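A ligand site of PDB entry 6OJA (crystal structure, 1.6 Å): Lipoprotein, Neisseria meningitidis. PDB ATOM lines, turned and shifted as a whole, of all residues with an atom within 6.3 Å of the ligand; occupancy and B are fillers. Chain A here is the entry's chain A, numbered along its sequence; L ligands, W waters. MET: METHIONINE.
N of Asn 199 is in hydrogen-bond range of OG1 of Thr 84 (2.8 Å). NH1 of Arg 117 lies within hydrogen-bond range of OD1 of Asn 114 (3.0 Å). ND2 of Asn 114 is in hydrogen-bond range of OD2 of Asp 111 (2.8 Å). ND2 of Asn 199 lies within hydrogen-bond range of O of Tyr 197 (2.9 Å). The backbone carbonyl oxygen (O) of Phe 59 lies close to the side-chain amide oxygen (OD1) of Asn 199. The side-chain amide oxygen of Asn 114 is in hydrogen-bond range of a ring nitrogen (NE2) of His 61, at 2.8 Å. NE2 of His 61 lies within hydrogen-bond range of NH1 of Arg 117, at 3.4 Å. The side-chain amide nitrogen of Asn 174 sits at hydrogen-bond distance from the side-chain amide oxygen of Asn 114 (3.3 Å).
SD of the ligand lies close to N of His 61, at 3.8 Å. NH1 of Arg 117 lies within salt-bridge range of O of the ligand. ND2 of Asn 114 lies close to SD of the ligand. The side-chain amide nitrogen of Asn 174 is in hydrogen-bond range of an oxygen (O) of the ligand, at 2.9 Å. N of the ligand is in hydrogen-bond range of OD1 of Asn 199, at 2.9 Å. A nitrogen (N) of the ligand lies within hydrogen-bond range of the side-chain amide oxygen (OD1) of Asn 176, 3.3 Å away. NE2 of His 61 sits close to SD of the ligand (3.4 Å).
Water W4 lies within hydrogen-bond range of OXT of the ligand (2.6 Å), NH2 of Arg 117 (2.8 Å), O of Tyr 197 (3.4 Å) and O of Ala 85 (3.4 Å). Water W3 lies within hydrogen-bond range of the backbone NH (N) of Gly 175 (2.7 Å), an oxygen (O) of the ligand (2.8 Å), the backbone NH (N) of Leu 87 (3.3 Å) and the backbone carbonyl oxygen (O) of Ala 85 (3.3 Å). Water W1 lies within hydrogen-bond range of a nitrogen (N) of the ligand (2.8 Å), the backbone carbonyl oxygen of Ala 85 (2.9 Å) and the backbone NH of Asn 176 (3.0 Å). Water W2 lies within hydrogen-bond range of the backbone carbonyl oxygen of Phe 59 (2.7 Å), the side-chain hydroxyl of Thr 11 (2.8 Å), a nitrogen (N) of the ligand (2.9 Å) and the side-chain amide oxygen of Asn 176 (3.3 Å).
CE2 of Phe 15 touches N of the ligand, at 3.9 Å. Tyr 42 touches the ligand. O of Phe 59 touches CB of the ligand, 3.3 Å away. Gln 60 touches the ligand (CB to CE, 3.7 Å). CB of Tyr 64 touches SD of the ligand, 3.5 Å away. Thr 84 touches the ligand. Tyr 197 touches the ligand. Hydrophobic or aromatic side chains within 4 Å of the ligand: Phe 15, Tyr 42, Phe 59, His 61 and Tyr 64. The nearest printed residue that does not touch the ligand is Ala 85 (4.3 Å).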
ATOM      1  N   THR A  11     -11.091  -4.180  -1.434  1.00  0.00           N
ATOM      2  CA  THR A  11     -11.072  -3.646  -0.082  1.00  0.00           C
ATOM      3  C   THR A  11     -12.488  -3.264   0.378  1.00  0.00           C
ATOM      4  O   THR A  11     -13.409  -3.087  -0.432  1.00  0.00           O
ATOM      5  CB  THR A  11     -10.126  -2.430   0.026  1.00  0.00           C
ATOM      6  OG1 THR A  11     -10.149  -1.659  -1.183  1.00  0.00           O
ATOM      7  CG2 THR A  11      -8.712  -2.872   0.278  1.00  0.00           C
ATOM      8  N   PHE A  15     -14.884   0.331  -3.246  1.00  0.00           N
ATOM      9  CA  PHE A  15     -14.766  -0.590  -4.383  1.00  0.00           C
ATOM     10  C   PHE A  15     -15.750  -1.753  -4.295  1.00  0.00           C
ATOM     11  O   PHE A  15     -16.214  -2.259  -5.332  1.00  0.00           O
ATOM     12  CB  PHE A  15     -13.347  -1.152  -4.457  1.00  0.00           C
ATOM     13  CG  PHE A  15     -12.314  -0.135  -4.866  1.00  0.00           C
ATOM     14  CD1 PHE A  15     -12.563   0.820  -5.847  1.00  0.00           C
ATOM     15  CD2 PHE A  15     -11.049  -0.156  -4.295  1.00  0.00           C
ATOM     16  CE1 PHE A  15     -11.589   1.734  -6.213  1.00  0.00           C
ATOM     17  CE2 PHE A  15     -10.081   0.750  -4.661  1.00  0.00           C
ATOM     18  CZ  PHE A  15     -10.340   1.687  -5.632  1.00  0.00           C
ATOM     19  N   TYR A  42      -4.011  -4.913   2.322  1.00  0.00           N
ATOM     20  CA  TYR A  42      -3.505  -4.856   0.959  1.00  0.00           C
ATOM     21  C   TYR A  42      -2.690  -6.087   0.539  1.00  0.00           C
ATOM     22  O   TYR A  42      -2.247  -6.150  -0.611  1.00  0.00           O
ATOM     23  CB  TYR A  42      -2.616  -3.623   0.792  1.00  0.00           C
ATOM     24  CG  TYR A  42      -3.266  -2.259   0.777  1.00  0.00           C
ATOM     25  CD1 TYR A  42      -4.616  -2.047   0.482  1.00  0.00           C
ATOM     26  CD2 TYR A  42      -2.462  -1.139   1.007  1.00  0.00           C
ATOM     27  CE1 TYR A  42      -5.127  -0.759   0.442  1.00  0.00           C
ATOM     28  CE2 TYR A  42      -2.968   0.121   0.955  1.00  0.00           C
ATOM     29  CZ  TYR A  42      -4.299   0.322   0.678  1.00  0.00           C
ATOM     30  OH  TYR A  42      -4.774   1.611   0.644  1.00  0.00           O
ATOM     31  N   PHE A  59      -8.483  -3.208  -6.027  1.00  0.00           N
ATOM     32  CA  PHE A  59      -8.073  -2.580  -4.790  1.00  0.00           C
ATOM     33  C   PHE A  59      -6.741  -1.847  -4.865  1.00  0.00           C
ATOM     34  O   PHE A  59      -6.379  -1.231  -3.875  1.00  0.00           O
ATOM     35  CB  PHE A  59      -7.964  -3.631  -3.668  1.00  0.00           C
ATOM     36  CG  PHE A  59      -6.653  -4.395  -3.678  1.00  0.00           C
ATOM     37  CD1 PHE A  59      -6.427  -5.413  -4.587  1.00  0.00           C
ATOM     38  CD2 PHE A  59      -5.630  -4.067  -2.792  1.00  0.00           C
ATOM     39  CE1 PHE A  59      -5.213  -6.104  -4.605  1.00  0.00           C
ATOM     40  CE2 PHE A  59      -4.445  -4.728  -2.806  1.00  0.00           C
ATOM     41  CZ  PHE A  59      -4.230  -5.763  -3.724  1.00  0.00           C
ATOM     42  N   GLN A  60      -6.017  -1.908  -5.972  1.00  0.00           N
ATOM     43  CA  GLN A  60      -4.625  -1.470  -5.972  1.00  0.00           C
ATOM     44  C   GLN A  60      -4.310  -0.616  -7.181  1.00  0.00           C
ATOM     45  O   GLN A  60      -5.020  -0.649  -8.199  1.00  0.00           O
ATOM     46  CB  GLN A  60      -3.674  -2.680  -5.951  1.00  0.00           C
ATOM     47  CG  GLN A  60      -3.558  -3.358  -7.301  1.00  0.00           C
ATOM     48  CD  GLN A  60      -3.099  -4.800  -7.180  1.00  0.00           C
ATOM     49  OE1 GLN A  60      -2.009  -5.090  -6.651  1.00  0.00           O
ATOM     50  NE2 GLN A  60      -3.927  -5.723  -7.652  1.00  0.00           N
ATOM     51  N   HIS A  61      -3.219   0.155  -7.081  1.00  0.00           N
ATOM     52  CA  HIS A  61      -2.677   0.833  -8.247  1.00  0.00           C
ATOM     53  C   HIS A  61      -1.573  -0.009  -8.893  1.00  0.00           C
ATOM     54  O   HIS A  61      -1.108  -1.029  -8.358  1.00  0.00           O
ATOM     55  CB  HIS A  61      -2.181   2.232  -7.889  1.00  0.00           C
ATOM     56  CG  HIS A  61      -1.320   2.317  -6.672  1.00  0.00           C
ATOM     57  ND1 HIS A  61      -0.049   1.794  -6.591  1.00  0.00           N
ATOM     58  CD2 HIS A  61      -1.548   2.943  -5.485  1.00  0.00           C
ATOM     59  CE1 HIS A  61       0.458   2.077  -5.404  1.00  0.00           C
ATOM     60  NE2 HIS A  61      -0.427   2.769  -4.714  1.00  0.00           N
ATOM     61  N   TYR A  64       1.874  -0.538  -7.142  1.00  0.00           N
ATOM     62  CA  TYR A  64       1.763  -1.561  -6.118  1.00  0.00           C
ATOM     63  C   TYR A  64       1.752  -2.953  -6.735  1.00  0.00           C
ATOM     64  O   TYR A  64       2.471  -3.852  -6.300  1.00  0.00           O
ATOM     65  CB  TYR A  64       0.502  -1.347  -5.256  1.00  0.00           C
ATOM     66  CG  TYR A  64       0.380  -2.301  -4.099  1.00  0.00           C
ATOM     67  CD1 TYR A  64      -0.217  -3.560  -4.242  1.00  0.00           C
ATOM     68  CD2 TYR A  64       0.887  -1.969  -2.871  1.00  0.00           C
ATOM     69  CE1 TYR A  64      -0.298  -4.434  -3.167  1.00  0.00           C
ATOM     70  CE2 TYR A  64       0.806  -2.821  -1.805  1.00  0.00           C
ATOM     71  CZ  TYR A  64       0.225  -4.055  -1.949  1.00  0.00           C
ATOM     72  OH  TYR A  64       0.213  -4.866  -0.828  1.00  0.00           O
ATOM     73  N   LEU A  65       0.917  -3.144  -7.776  1.00  0.00           N
ATOM     74  CA  LEU A  65       0.772  -4.441  -8.417  1.00  0.00           C
ATOM     75  C   LEU A  65       2.088  -4.895  -9.040  1.00  0.00           C
ATOM     76  O   LEU A  65       2.494  -6.054  -8.875  1.00  0.00           O
ATOM     77  CB  LEU A  65      -0.298  -4.356  -9.497  1.00  0.00           C
ATOM     78  CG  LEU A  65      -0.490  -5.594 -10.362  1.00  0.00           C
ATOM     79  CD1 LEU A  65      -0.886  -6.823  -9.559  1.00  0.00           C
ATOM     80  CD2 LEU A  65      -1.522  -5.297 -11.439  1.00  0.00           C
ATOM     81  N   THR A  84     -11.176   6.170  -8.423  1.00  0.00           N
ATOM     82  CA  THR A  84     -10.284   5.962  -7.290  1.00  0.00           C
ATOM     83  C   THR A  84     -10.252   7.161  -6.360  1.00  0.00           C
ATOM     84  O   THR A  84     -10.041   8.291  -6.797  1.00  0.00           O
ATOM     85  CB  THR A  84      -8.863   5.693  -7.807  1.00  0.00           C
ATOM     86  OG1 THR A  84      -8.886   4.504  -8.607  1.00  0.00           O
ATOM     87  CG2 THR A  84      -7.865   5.502  -6.673  1.00  0.00           C
ATOM     88  N   ALA A  85     -10.461   6.892  -5.072  1.00  0.00           N
ATOM     89  CA  ALA A  85     -10.313   7.938  -4.058  1.00  0.00           C
ATOM     90  C   ALA A  85      -8.849   8.380  -3.984  1.00  0.00           C
ATOM     91  O   ALA A  85      -7.947   7.536  -3.806  1.00  0.00           O
ATOM     92  CB  ALA A  85     -10.806   7.448  -2.689  1.00  0.00           C
ATOM     93  N   PRO A  86      -8.568   9.676  -4.100  1.00  0.00           N
ATOM     94  CA  PRO A  86      -7.179  10.151  -4.128  1.00  0.00           C
ATOM     95  C   PRO A  86      -6.526  10.123  -2.755  1.00  0.00           C
ATOM     96  O   PRO A  86      -7.162   9.996  -1.713  1.00  0.00           O
ATOM     97  CB  PRO A  86      -7.286  11.584  -4.645  1.00  0.00           C
ATOM     98  CG  PRO A  86      -8.683  11.985  -4.327  1.00  0.00           C
ATOM     99  CD  PRO A  86      -9.523  10.752  -4.356  1.00  0.00           C
ATOM    100  N   LEU A  87      -5.207  10.263  -2.797  1.00  0.00           N
ATOM    101  CA  LEU A  87      -4.380  10.320  -1.619  1.00  0.00           C
ATOM    102  C   LEU A  87      -4.361  11.741  -1.083  1.00  0.00           C
ATOM    103  O   LEU A  87      -4.227  12.697  -1.849  1.00  0.00           O
ATOM    104  CB  LEU A  87      -2.958   9.891  -1.971  1.00  0.00           C
ATOM    105  CG  LEU A  87      -1.958   9.757  -0.825  1.00  0.00           C
ATOM    106  CD1 LEU A  87      -2.298   8.553   0.024  1.00  0.00           C
ATOM    107  CD2 LEU A  87      -0.557   9.653  -1.386  1.00  0.00           C
ATOM    108  N   ASP A 111       4.569   0.365   3.050  1.00  0.00           N
ATOM    109  CA  ASP A 111       4.905  -0.456   1.916  1.00  0.00           C
ATOM    110  C   ASP A 111       5.556   0.415   0.846  1.00  0.00           C
ATOM    111  O   ASP A 111       5.261   1.602   0.762  1.00  0.00           O
ATOM    112  CB  ASP A 111       3.659  -1.143   1.361  1.00  0.00           C
ATOM    113  CG  ASP A 111       2.605  -0.165   0.891  1.00  0.00           C
ATOM    114  OD1 ASP A 111       1.906   0.475   1.723  1.00  0.00           O
ATOM    115  OD2 ASP A 111       2.517  -0.003  -0.332  1.00  0.00           O
ATOM    116  N   SER A 113       5.667   1.123  -2.540  1.00  0.00           N
ATOM    117  CA  SER A 113       5.077   1.946  -3.592  1.00  0.00           C
ATOM    118  C   SER A 113       4.210   3.062  -3.011  1.00  0.00           C
ATOM    119  O   SER A 113       4.125   4.149  -3.601  1.00  0.00           O
ATOM    120  CB  SER A 113       4.281   1.095  -4.598  1.00  0.00           C
ATOM    121  OG  SER A 113       3.106   0.561  -4.039  1.00  0.00           O
ATOM    122  N   ASN A 114       3.526   2.826  -1.887  1.00  0.00           N
ATOM    123  CA  ASN A 114       2.733   3.885  -1.274  1.00  0.00           C
ATOM    124  C   ASN A 114       3.615   4.831  -0.454  1.00  0.00           C
ATOM    125  O   ASN A 114       3.336   6.035  -0.389  1.00  0.00           O
ATOM    126  CB  ASN A 114       1.618   3.262  -0.442  1.00  0.00           C
ATOM    127  CG  ASN A 114       0.517   2.735  -1.318  1.00  0.00           C
ATOM    128  OD1 ASN A 114      -0.137   3.503  -2.014  1.00  0.00           O
ATOM    129  ND2 ASN A 114       0.365   1.424  -1.345  1.00  0.00           N
ATOM    130  N   ARG A 117       4.898   7.673  -2.578  1.00  0.00           N
ATOM    131  CA  ARG A 117       3.924   8.750  -2.802  1.00  0.00           C
ATOM    132  C   ARG A 117       4.025   9.804  -1.722  1.00  0.00           C
ATOM    133  O   ARG A 117       3.801  10.987  -1.995  1.00  0.00           O
ATOM    134  CB  ARG A 117       2.522   8.188  -2.825  1.00  0.00           C
ATOM    135  CG  ARG A 117       2.319   7.163  -3.904  1.00  0.00           C
ATOM    136  CD  ARG A 117       1.014   6.416  -3.721  1.00  0.00           C
ATOM    137  NE  ARG A 117      -0.125   7.213  -4.149  1.00  0.00           N
ATOM    138  CZ  ARG A 117      -1.392   6.819  -4.019  1.00  0.00           C
ATOM    139  NH1 ARG A 117      -1.661   5.659  -3.417  1.00  0.00           N
ATOM    140  NH2 ARG A 117      -2.381   7.579  -4.492  1.00  0.00           N
ATOM    141  N   ASN A 174      -4.463   6.748   2.527  1.00  0.00           N
ATOM    142  CA  ASN A 174      -4.973   6.229   1.263  1.00  0.00           C
ATOM    143  C   ASN A 174      -6.472   6.446   1.193  1.00  0.00           C
ATOM    144  O   ASN A 174      -7.185   6.261   2.191  1.00  0.00           O
ATOM    145  CB  ASN A 174      -4.665   4.745   1.136  1.00  0.00           C
ATOM    146  CG  ASN A 174      -3.176   4.459   1.083  1.00  0.00           C
ATOM    147  OD1 ASN A 174      -2.520   4.254   2.109  1.00  0.00           O
ATOM    148  ND2 ASN A 174      -2.626   4.422  -0.117  1.00  0.00           N
ATOM    149  N   GLY A 175      -6.963   6.791   0.005  1.00  0.00           N
ATOM    150  CA  GLY A 175      -8.352   7.175  -0.130  1.00  0.00           C
ATOM    151  C   GLY A 175      -9.317   6.118   0.372  1.00  0.00           C
ATOM    152  O   GLY A 175     -10.315   6.431   1.021  1.00  0.00           O
ATOM    153  N   ASN A 176      -9.066   4.841   0.055  1.00  0.00           N
ATOM    154  CA  ASN A 176     -10.046   3.837   0.440  1.00  0.00           C
ATOM    155  C   ASN A 176     -10.204   3.779   1.951  1.00  0.00           C
ATOM    156  O   ASN A 176     -11.327   3.600   2.455  1.00  0.00           O
ATOM    157  CB  ASN A 176      -9.673   2.455  -0.093  1.00  0.00           C
ATOM    158  CG  ASN A 176      -8.397   1.919   0.501  1.00  0.00           C
ATOM    159  OD1 ASN A 176      -7.296   2.388   0.178  1.00  0.00           O
ATOM    160  ND2 ASN A 176      -8.529   0.942   1.397  1.00  0.00           N
ATOM    161  N   TYR A 197      -1.714   6.745  -9.951  1.00  0.00           N
ATOM    162  CA  TYR A 197      -2.175   5.811  -8.951  1.00  0.00           C
ATOM    163  C   TYR A 197      -3.671   5.543  -9.026  1.00  0.00           C
ATOM    164  O   TYR A 197      -4.250   5.013  -8.073  1.00  0.00           O
ATOM    165  CB  TYR A 197      -1.771   6.306  -7.557  1.00  0.00           C
ATOM    166  CG  TYR A 197      -0.274   6.398  -7.437  1.00  0.00           C
ATOM    167  CD1 TYR A 197       0.493   5.250  -7.186  1.00  0.00           C
ATOM    168  CD2 TYR A 197       0.393   7.603  -7.624  1.00  0.00           C
ATOM    169  CE1 TYR A 197       1.862   5.328  -7.074  1.00  0.00           C
ATOM    170  CE2 TYR A 197       1.779   7.670  -7.514  1.00  0.00           C
ATOM    171  CZ  TYR A 197       2.496   6.555  -7.257  1.00  0.00           C
ATOM    172  OH  TYR A 197       3.885   6.666  -7.146  1.00  0.00           O
ATOM    173  N   VAL A 198      -4.322   5.884 -10.139  1.00  0.00           N
ATOM    174  CA  VAL A 198      -5.687   5.435 -10.353  1.00  0.00           C
ATOM    175  C   VAL A 198      -5.690   3.912 -10.391  1.00  0.00           C
ATOM    176  O   VAL A 198      -4.885   3.282 -11.082  1.00  0.00           O
ATOM    177  CB  VAL A 198      -6.243   6.054 -11.637  1.00  0.00           C
ATOM    178  CG1 VAL A 198      -7.644   5.507 -11.941  1.00  0.00           C
ATOM    179  CG2 VAL A 198      -6.294   7.589 -11.513  1.00  0.00           C
ATOM    180  N   ASN A 199      -6.580   3.300  -9.622  1.00  0.00           N
ATOM    181  CA  ASN A 199      -6.499   1.875  -9.373  1.00  0.00           C
ATOM    182  C   ASN A 199      -6.925   1.045 -10.575  1.00  0.00           C
ATOM    183  O   ASN A 199      -7.681   1.495 -11.442  1.00  0.00           O
ATOM    184  CB  ASN A 199      -7.326   1.508  -8.159  1.00  0.00           C
ATOM    185  CG  ASN A 199      -6.684   1.887  -6.842  1.00  0.00           C
ATOM    186  OD1 ASN A 199      -7.100   1.410  -5.792  1.00  0.00           O
ATOM    187  ND2 ASN A 199      -5.688   2.795  -6.879  1.00  0.00           N
HETATM  188  N   MET L   1      -6.842   2.317  -3.084  1.00  0.00           N
HETATM  189  CA  MET L   1      -5.436   2.510  -2.671  1.00  0.00           C
HETATM  190  C   MET L   1      -4.950   3.831  -3.198  1.00  0.00           C
HETATM  191  O   MET L   1      -4.213   4.557  -2.532  1.00  0.00           O
HETATM  192  CB  MET L   1      -4.564   1.393  -3.203  1.00  0.00           C
HETATM  193  CG  MET L   1      -3.132   1.488  -2.745  1.00  0.00           C
HETATM  194  SD  MET L   1      -2.128   0.141  -3.457  1.00  0.00           S
HETATM  195  CE  MET L   1      -2.824  -1.301  -2.652  1.00  0.00           C
HETATM  196  OXT MET L   1      -5.312   4.203  -4.338  1.00  0.00           O
HETATM  197  O   HOH W   1      -8.273   4.756  -2.878  1.00  0.00           O
HETATM  198  O   HOH W   2      -7.886  -0.123  -1.895  1.00  0.00           O
HETATM  199  O   HOH W   3      -5.215   7.087  -2.094  1.00  0.00           O
HETATM  200  O   HOH W   4      -4.948   6.618  -5.210  1.00  0.00           O
